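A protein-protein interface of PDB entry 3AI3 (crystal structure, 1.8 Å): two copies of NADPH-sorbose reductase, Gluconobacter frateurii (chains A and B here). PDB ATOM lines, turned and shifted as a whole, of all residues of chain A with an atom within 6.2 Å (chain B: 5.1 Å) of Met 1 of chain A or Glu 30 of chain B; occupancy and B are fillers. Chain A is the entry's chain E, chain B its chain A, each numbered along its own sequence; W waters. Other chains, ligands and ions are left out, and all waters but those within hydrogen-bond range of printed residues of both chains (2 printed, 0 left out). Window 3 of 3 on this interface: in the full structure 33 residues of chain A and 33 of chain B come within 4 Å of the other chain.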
ATOM      1  N   MET A   1     -22.499 -28.171   2.800  1.00  0.00           N
ATOM      2  CA  MET A   1     -22.553 -28.010   4.289  1.00  0.00           C
ATOM      3  C   MET A   1     -21.202 -28.444   4.836  1.00  0.00           C
ATOM      4  O   MET A   1     -20.759 -29.550   4.556  1.00  0.00           O
ATOM      5  CB  MET A   1     -23.665 -28.878   4.894  1.00  0.00           C
ATOM      6  CG  MET A   1     -23.841 -28.687   6.399  1.00  0.00           C
ATOM      7  SD  MET A   1     -25.054 -29.811   7.130  1.00  0.00           S
ATOM      8  CE  MET A   1     -26.557 -28.924   6.818  1.00  0.00           C
ATOM      9  N   ASP A   2     -20.546 -27.574   5.599  1.00  0.00           N
ATOM     10  CA  ASP A   2     -19.228 -27.899   6.143  1.00  0.00           C
ATOM     11  C   ASP A   2     -19.362 -28.916   7.284  1.00  0.00           C
ATOM     12  O   ASP A   2     -20.136 -28.703   8.208  1.00  0.00           O
ATOM     13  CB  ASP A   2     -18.536 -26.630   6.645  1.00  0.00           C
ATOM     14  CG  ASP A   2     -18.157 -25.686   5.524  1.00  0.00           C
ATOM     15  OD1 ASP A   2     -18.233 -26.073   4.332  1.00  0.00           O
ATOM     16  OD2 ASP A   2     -17.770 -24.541   5.842  1.00  0.00           O
ATOM     17  N   MET A   3     -18.602 -30.007   7.225  1.00  0.00           N
ATOM     18  CA  MET A   3     -18.730 -31.076   8.232  1.00  0.00           C
ATOM     19  C   MET A   3     -17.758 -30.920   9.416  1.00  0.00           C
ATOM     20  O   MET A   3     -18.008 -31.462  10.503  1.00  0.00           O
ATOM     21  CB  MET A   3     -18.514 -32.443   7.584  1.00  0.00           C
ATOM     22  CG  MET A   3     -19.569 -32.834   6.555  1.00  0.00           C
ATOM     23  SD  MET A   3     -21.143 -33.302   7.313  1.00  0.00           S
ATOM     24  CE  MET A   3     -22.044 -31.809   7.016  1.00  0.00           C
ATOM     25  N   GLU A  30     -13.987 -36.159   3.466  1.00  0.00           N
ATOM     26  CA  GLU A  30     -14.110 -34.990   4.317  1.00  0.00           C
ATOM     27  C   GLU A  30     -12.794 -34.695   5.024  1.00  0.00           C
ATOM     28  O   GLU A  30     -12.734 -33.841   5.909  1.00  0.00           O
ATOM     29  CB  GLU A  30     -15.235 -35.195   5.349  1.00  0.00           C
ATOM     30  CG  GLU A  30     -16.657 -35.049   4.769  1.00  0.00           C
ATOM     31  CD  GLU A  30     -16.967 -33.635   4.319  1.00  0.00           C
ATOM     32  OE1 GLU A  30     -16.325 -32.696   4.823  1.00  0.00           O
ATOM     33  OE2 GLU A  30     -17.847 -33.456   3.450  1.00  0.00           O
ATOM     34  N   PHE A 239     -22.510 -37.411   8.559  1.00  0.00           N
ATOM     35  CA  PHE A 239     -23.249 -36.312   9.132  1.00  0.00           C
ATOM     36  C   PHE A 239     -23.338 -36.408  10.660  1.00  0.00           C
ATOM     37  O   PHE A 239     -23.066 -35.425  11.365  1.00  0.00           O
ATOM     38  CB  PHE A 239     -24.638 -36.208   8.491  1.00  0.00           C
ATOM     39  CG  PHE A 239     -25.495 -35.173   9.133  1.00  0.00           C
ATOM     40  CD1 PHE A 239     -25.305 -33.841   8.844  1.00  0.00           C
ATOM     41  CD2 PHE A 239     -26.485 -35.541  10.036  1.00  0.00           C
ATOM     42  CE1 PHE A 239     -26.085 -32.844   9.474  1.00  0.00           C
ATOM     43  CE2 PHE A 239     -27.249 -34.578  10.681  1.00  0.00           C
ATOM     44  CZ  PHE A 239     -27.058 -33.230  10.403  1.00  0.00           C
ATOM     45  N   SER A 242     -20.319 -35.347  12.609  1.00  0.00           N
ATOM     46  CA  SER A 242     -19.800 -34.061  12.148  1.00  0.00           C
ATOM     47  C   SER A 242     -20.076 -32.959  13.165  1.00  0.00           C
ATOM     48  O   SER A 242     -20.830 -33.151  14.134  1.00  0.00           O
ATOM     49  CB  SER A 242     -20.444 -33.649  10.817  1.00  0.00           C
ATOM     50  OG  SER A 242     -21.727 -33.070  11.042  1.00  0.00           O
ATOM     51  N   ARG A 244     -21.942 -30.709  12.663  1.00  0.00           N
ATOM     52  CA  ARG A 244     -23.316 -30.235  12.395  1.00  0.00           C
ATOM     53  C   ARG A 244     -24.384 -31.027  13.162  1.00  0.00           C
ATOM     54  O   ARG A 244     -25.569 -30.707  13.070  1.00  0.00           O
ATOM     55  CB  ARG A 244     -23.636 -30.330  10.892  1.00  0.00           C
ATOM     56  CG  ARG A 244     -22.672 -29.551   9.992  1.00  0.00           C
ATOM     57  CD  ARG A 244     -22.951 -28.043   9.932  1.00  0.00           C
ATOM     58  NE  ARG A 244     -22.516 -27.281  11.118  1.00  0.00           N
ATOM     59  CZ  ARG A 244     -21.249 -27.002  11.429  1.00  0.00           C
ATOM     60  NH1 ARG A 244     -20.241 -27.451  10.677  1.00  0.00           N
ATOM     61  NH2 ARG A 244     -20.978 -26.265  12.513  1.00  0.00           N
ATOM     62  N   MET B   1     -19.637 -31.380   2.649  1.00  0.00           N
ATOM     63  CA  MET B   1     -20.571 -32.333   1.984  1.00  0.00           C
ATOM     64  C   MET B   1     -21.572 -31.539   1.175  1.00  0.00           C
ATOM     65  O   MET B   1     -22.287 -30.705   1.721  1.00  0.00           O
ATOM     66  CB  MET B   1     -21.328 -33.175   3.010  1.00  0.00           C
ATOM     67  CG  MET B   1     -22.187 -34.287   2.391  1.00  0.00           C
ATOM     68  SD  MET B   1     -23.128 -35.233   3.630  1.00  0.00           S
ATOM     69  CE  MET B   1     -21.819 -36.207   4.364  1.00  0.00           C
ATOM     70  N   ASP B   2     -21.619 -31.826  -0.120  1.00  0.00           N
ATOM     71  CA  ASP B   2     -22.564 -31.179  -1.026  1.00  0.00           C
ATOM     72  C   ASP B   2     -23.960 -31.688  -0.717  1.00  0.00           C
ATOM     73  O   ASP B   2     -24.191 -32.893  -0.673  1.00  0.00           O
ATOM     74  CB  ASP B   2     -22.196 -31.497  -2.476  1.00  0.00           C
ATOM     75  CG  ASP B   2     -23.107 -30.795  -3.508  1.00  0.00           C
ATOM     76  OD1 ASP B   2     -23.863 -29.858  -3.163  1.00  0.00           O
ATOM     77  OD2 ASP B   2     -23.058 -31.194  -4.702  1.00  0.00           O
ATOM     78  N   MET B   3     -24.879 -30.760  -0.501  1.00  0.00           N
ATOM     79  CA  MET B   3     -26.270 -31.100  -0.195  1.00  0.00           C
ATOM     80  C   MET B   3     -27.128 -31.296  -1.456  1.00  0.00           C
ATOM     81  O   MET B   3     -28.178 -31.939  -1.408  1.00  0.00           O
ATOM     82  CB  MET B   3     -26.884 -30.039   0.722  1.00  0.00           C
ATOM     83  CG  MET B   3     -26.328 -30.006   2.130  1.00  0.00           C
ATOM     84  SD  MET B   3     -26.636 -31.507   3.100  1.00  0.00           S
ATOM     85  CE  MET B   3     -25.008 -32.212   3.090  1.00  0.00           C
ATOM     86  N   ILE B   5     -28.925 -29.166  -3.195  1.00  0.00           N
ATOM     87  CA  ILE B   5     -30.244 -28.513  -3.186  1.00  0.00           C
ATOM     88  C   ILE B   5     -30.214 -27.098  -3.748  1.00  0.00           C
ATOM     89  O   ILE B   5     -31.171 -26.330  -3.574  1.00  0.00           O
ATOM     90  CB  ILE B   5     -30.936 -28.532  -1.799  1.00  0.00           C
ATOM     91  CG1 ILE B   5     -30.131 -27.755  -0.768  1.00  0.00           C
ATOM     92  CG2 ILE B   5     -31.179 -29.962  -1.313  1.00  0.00           C
ATOM     93  CD1 ILE B   5     -30.848 -27.672   0.591  1.00  0.00           C
ATOM     94  N   SER B   6     -29.124 -26.756  -4.436  1.00  0.00           N
ATOM     95  CA  SER B   6     -28.991 -25.401  -4.978  1.00  0.00           C
ATOM     96  C   SER B   6     -30.096 -25.150  -5.996  1.00  0.00           C
ATOM     97  O   SER B   6     -30.296 -25.966  -6.883  1.00  0.00           O
ATOM     98  CB  SER B   6     -27.629 -25.233  -5.681  1.00  0.00           C
ATOM     99  OG  SER B   6     -27.574 -23.921  -6.201  1.00  0.00           O
ATOM    100  N   GLY B  26     -30.632 -22.122   6.933  1.00  0.00           N
ATOM    101  CA  GLY B  26     -29.876 -23.338   6.573  1.00  0.00           C
ATOM    102  C   GLY B  26     -30.037 -23.705   5.087  1.00  0.00           C
ATOM    103  O   GLY B  26     -29.057 -24.083   4.414  1.00  0.00           O
ATOM    104  N   PHE B  27     -31.266 -23.637   4.584  1.00  0.00           N
ATOM    105  CA  PHE B  27     -31.537 -24.033   3.213  1.00  0.00           C
ATOM    106  C   PHE B  27     -30.948 -22.979   2.269  1.00  0.00           C
ATOM    107  O   PHE B  27     -30.342 -23.320   1.260  1.00  0.00           O
ATOM    108  CB  PHE B  27     -33.048 -24.164   2.948  1.00  0.00           C
ATOM    109  CG  PHE B  27     -33.640 -25.470   3.391  1.00  0.00           C
ATOM    110  CD1 PHE B  27     -33.174 -26.679   2.861  1.00  0.00           C
ATOM    111  CD2 PHE B  27     -34.689 -25.507   4.288  1.00  0.00           C
ATOM    112  CE1 PHE B  27     -33.726 -27.891   3.239  1.00  0.00           C
ATOM    113  CE2 PHE B  27     -35.256 -26.745   4.686  1.00  0.00           C
ATOM    114  CZ  PHE B  27     -34.755 -27.933   4.164  1.00  0.00           C
ATOM    115  N   ALA B  28     -31.107 -21.712   2.637  1.00  0.00           N
ATOM    116  CA  ALA B  28     -30.591 -20.581   1.827  1.00  0.00           C
ATOM    117  C   ALA B  28     -29.056 -20.657   1.706  1.00  0.00           C
ATOM    118  O   ALA B  28     -28.485 -20.400   0.649  1.00  0.00           O
ATOM    119  CB  ALA B  28     -31.035 -19.249   2.442  1.00  0.00           C
ATOM    120  N   LYS B  29     -28.400 -21.056   2.784  1.00  0.00           N
ATOM    121  CA  LYS B  29     -26.932 -21.247   2.759  1.00  0.00           C
ATOM    122  C   LYS B  29     -26.506 -22.296   1.737  1.00  0.00           C
ATOM    123  O   LYS B  29     -25.399 -22.234   1.190  1.00  0.00           O
ATOM    124  CB  LYS B  29     -26.443 -21.629   4.148  1.00  0.00           C
ATOM    125  CG  LYS B  29     -24.908 -21.556   4.344  1.00  0.00           C
ATOM    126  CD  LYS B  29     -24.528 -21.934   5.771  1.00  0.00           C
ATOM    127  CE  LYS B  29     -25.283 -21.122   6.817  1.00  0.00           C
ATOM    128  NZ  LYS B  29     -24.778 -21.393   8.208  1.00  0.00           N
ATOM    129  N   GLU B  30     -27.378 -23.267   1.496  1.00  0.00           N
ATOM    130  CA  GLU B  30     -27.120 -24.301   0.491  1.00  0.00           C
ATOM    131  C   GLU B  30     -27.666 -23.941  -0.907  1.00  0.00           C
ATOM    132  O   GLU B  30     -27.589 -24.735  -1.844  1.00  0.00           O
ATOM    133  CB  GLU B  30     -27.628 -25.661   0.970  1.00  0.00           C
ATOM    134  CG  GLU B  30     -27.149 -26.075   2.403  1.00  0.00           C
ATOM    135  CD  GLU B  30     -25.627 -26.131   2.597  1.00  0.00           C
ATOM    136  OE1 GLU B  30     -24.908 -26.705   1.755  1.00  0.00           O
ATOM    137  OE2 GLU B  30     -25.147 -25.602   3.630  1.00  0.00           O
ATOM    138  N   GLY B  31     -28.192 -22.732  -1.049  1.00  0.00           N
ATOM    139  CA  GLY B  31     -28.555 -22.216  -2.367  1.00  0.00           C
ATOM    140  C   GLY B  31     -30.007 -22.405  -2.767  1.00  0.00           C
ATOM    141  O   GLY B  31     -30.379 -22.100  -3.899  1.00  0.00           O
ATOM    142  N   ALA B  32     -30.829 -22.906  -1.841  1.00  0.00           N
ATOM    143  CA  ALA B  32     -32.260 -23.078  -2.087  1.00  0.00           C
ATOM    144  C   ALA B  32     -33.029 -21.769  -1.980  1.00  0.00           C
ATOM    145  O   ALA B  32     -32.791 -20.959  -1.068  1.00  0.00           O
ATOM    146  CB  ALA B  32     -32.860 -24.102  -1.099  1.00  0.00           C
ATOM    147  N   ASN B 235     -29.543 -27.772  11.035  1.00  0.00           N
ATOM    148  CA  ASN B 235     -28.656 -28.651  10.242  1.00  0.00           C
ATOM    149  C   ASN B 235     -29.315 -29.973   9.892  1.00  0.00           C
ATOM    150  O   ASN B 235     -29.141 -30.479   8.793  1.00  0.00           O
ATOM    151  CB  ASN B 235     -27.355 -28.943  10.987  1.00  0.00           C
ATOM    152  CG  ASN B 235     -26.529 -27.698  11.216  1.00  0.00           C
ATOM    153  OD1 ASN B 235     -26.516 -26.799  10.377  1.00  0.00           O
ATOM    154  ND2 ASN B 235     -25.822 -27.640  12.353  1.00  0.00           N
ATOM    155  N   VAL B 238     -31.888 -29.637   7.062  1.00  0.00           N
ATOM    156  CA  VAL B 238     -31.220 -29.436   5.765  1.00  0.00           C
ATOM    157  C   VAL B 238     -30.682 -30.765   5.272  1.00  0.00           C
ATOM    158  O   VAL B 238     -30.972 -31.158   4.138  1.00  0.00           O
ATOM    159  CB  VAL B 238     -30.116 -28.377   5.835  1.00  0.00           C
ATOM    160  CG1 VAL B 238     -29.455 -28.211   4.492  1.00  0.00           C
ATOM    161  CG2 VAL B 238     -30.698 -27.013   6.274  1.00  0.00           C
ATOM    162  N   PHE B 239     -29.971 -31.489   6.133  1.00  0.00           N
ATOM    163  CA  PHE B 239     -29.501 -32.832   5.758  1.00  0.00           C
ATOM    164  C   PHE B 239     -30.644 -33.723   5.297  1.00  0.00           C
ATOM    165  O   PHE B 239     -30.559 -34.345   4.221  1.00  0.00           O
ATOM    166  CB  PHE B 239     -28.701 -33.494   6.901  1.00  0.00           C
ATOM    167  CG  PHE B 239     -28.207 -34.851   6.557  1.00  0.00           C
ATOM    168  CD1 PHE B 239     -27.087 -35.001   5.738  1.00  0.00           C
ATOM    169  CD2 PHE B 239     -28.896 -35.980   6.997  1.00  0.00           C
ATOM    170  CE1 PHE B 239     -26.639 -36.293   5.381  1.00  0.00           C
ATOM    171  CE2 PHE B 239     -28.461 -37.267   6.644  1.00  0.00           C
ATOM    172  CZ  PHE B 239     -27.328 -37.414   5.838  1.00  0.00           C
HETATM  173  O   HOH W   1     -24.089 -25.726  13.300  1.00  0.00           O
HETATM  174  O   HOH W   2     -17.128 -30.352   4.801  1.00  0.00           O
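The backbone carbonyl oxygen (O) of Met 1 of chain B lies within hydrogen-bond range of the backbone NH (N) of Met 1 of chain A.
The side-chain amide nitrogen (ND2) of Asn 235 of chain B lies within hydrogen-bond range of the backbone carbonyl oxygen (O) of Arg 244 of chain A, at 3.2 Å.
The side-chain carboxylate of Glu 30 of chain B sits at hydrogen-bond distance from the backbone NH of Met 1 of chain A, 3.0 Å away.
The side-chain carboxylate (OE2) of Glu 30 of chain A lies within hydrogen-bond range of the backbone NH (N) of Met 1 of chain B, 2.9 Å away.
The side-chain sulfur (SD) of Met 3 of chain A lies close to the side-chain hydroxyl (OG) of Ser 242 of chain A, at 3.8 Å.
The backbone NH (N) of Arg 244 of chain A is in hydrogen-bond range of the side-chain hydroxyl (OG) of Ser 242 of chain A, at 2.9 Å.
The backbone carbonyl oxygen of Asp 2 of chain A lies within hydrogen-bond range of the guanidinium group of Arg 244 of chain A.
The backbone carbonyl oxygen (O) of Phe 239 of chain A is in hydrogen-bond range of the side-chain hydroxyl (OG) of Ser 242 of chain A (2.7 Å).
Among the printed residues, pairs that only touch across the chains: Met 1 of chain A with Asn 235 of chain B (3.6 Å), Met 1 of chain A with Val 238 of chain B (3.7 Å), Met 3 of chain A with Met 1 of chain B (3.97 Å), Phe 239 of chain A with Asn 235 of chain B (3.8 Å) and Phe 239 of chain A with Phe 239 of chain B (3.7 Å).
Of chain A, only Met 1 (3.0 Å) comes within 4 Å of Glu 30 of chain B.
Of the printed residues of chain B, Phe 239 of chain A touches Asn 235 and Phe 239.
Of the printed residues of chain B, Met 3 of chain A touches Met 1 (3.97 Å).
Asp 2 of chain A touches none of the printed residues of chain B.
Ser 6 of chain B touches none of the printed residues of chain A.
The nearest printed residue of chain B that does not touch Met 1 of chain A is Met 3 of chain B (4.0005 Å).
The nearest residue of chain A that does not touch Glu 30 of chain B is Asp 2 of chain A (5.4 Å).
Of the 7 printed residues of chain A, 5 touch a printed residue of chain B.
Printed residues of chain A that touch a printed residue of chain B: Met 1, Met 3, Glu 30, Phe 239 and Arg 244.
Among the printed residues, 9 pairs touch across the chains.
Met 1 of chain A touches its own counterpart, Met 1 of chain B.
Met 1 of chain A touches Glu 30 of chain B, and with the chains exchanged Glu 30 of chain A touches Met 1 of chain B.
Met 3 of chain A touches Met 1 of chain B, but with the chains exchanged Met 1 of chain A does not touch Met 3 of chain B (4.0005 Å).
Phe 239 of chain B touches its own counterpart, Phe 239 of chain A.
Positions printed for both chains: 1, 2, 3, 30 and 239.
Of the 9 pairs that touch across the chains among the printed residues, 4 have their exchanged pair printed and touching as well.
Water W2 lies within hydrogen-bond range of OE1 of Glu 30 of chain A (2.5 Å), N of Met 3 of chain A (2.9 Å) and N of Met 1 of chain B (3.5 Å).
Water W1 bridges the side-chain amide nitrogen (ND2) of Asn 235 of chain B (2.8 Å) and the guanidinium group (NE) of Arg 244 of chain A (3.1 Å).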
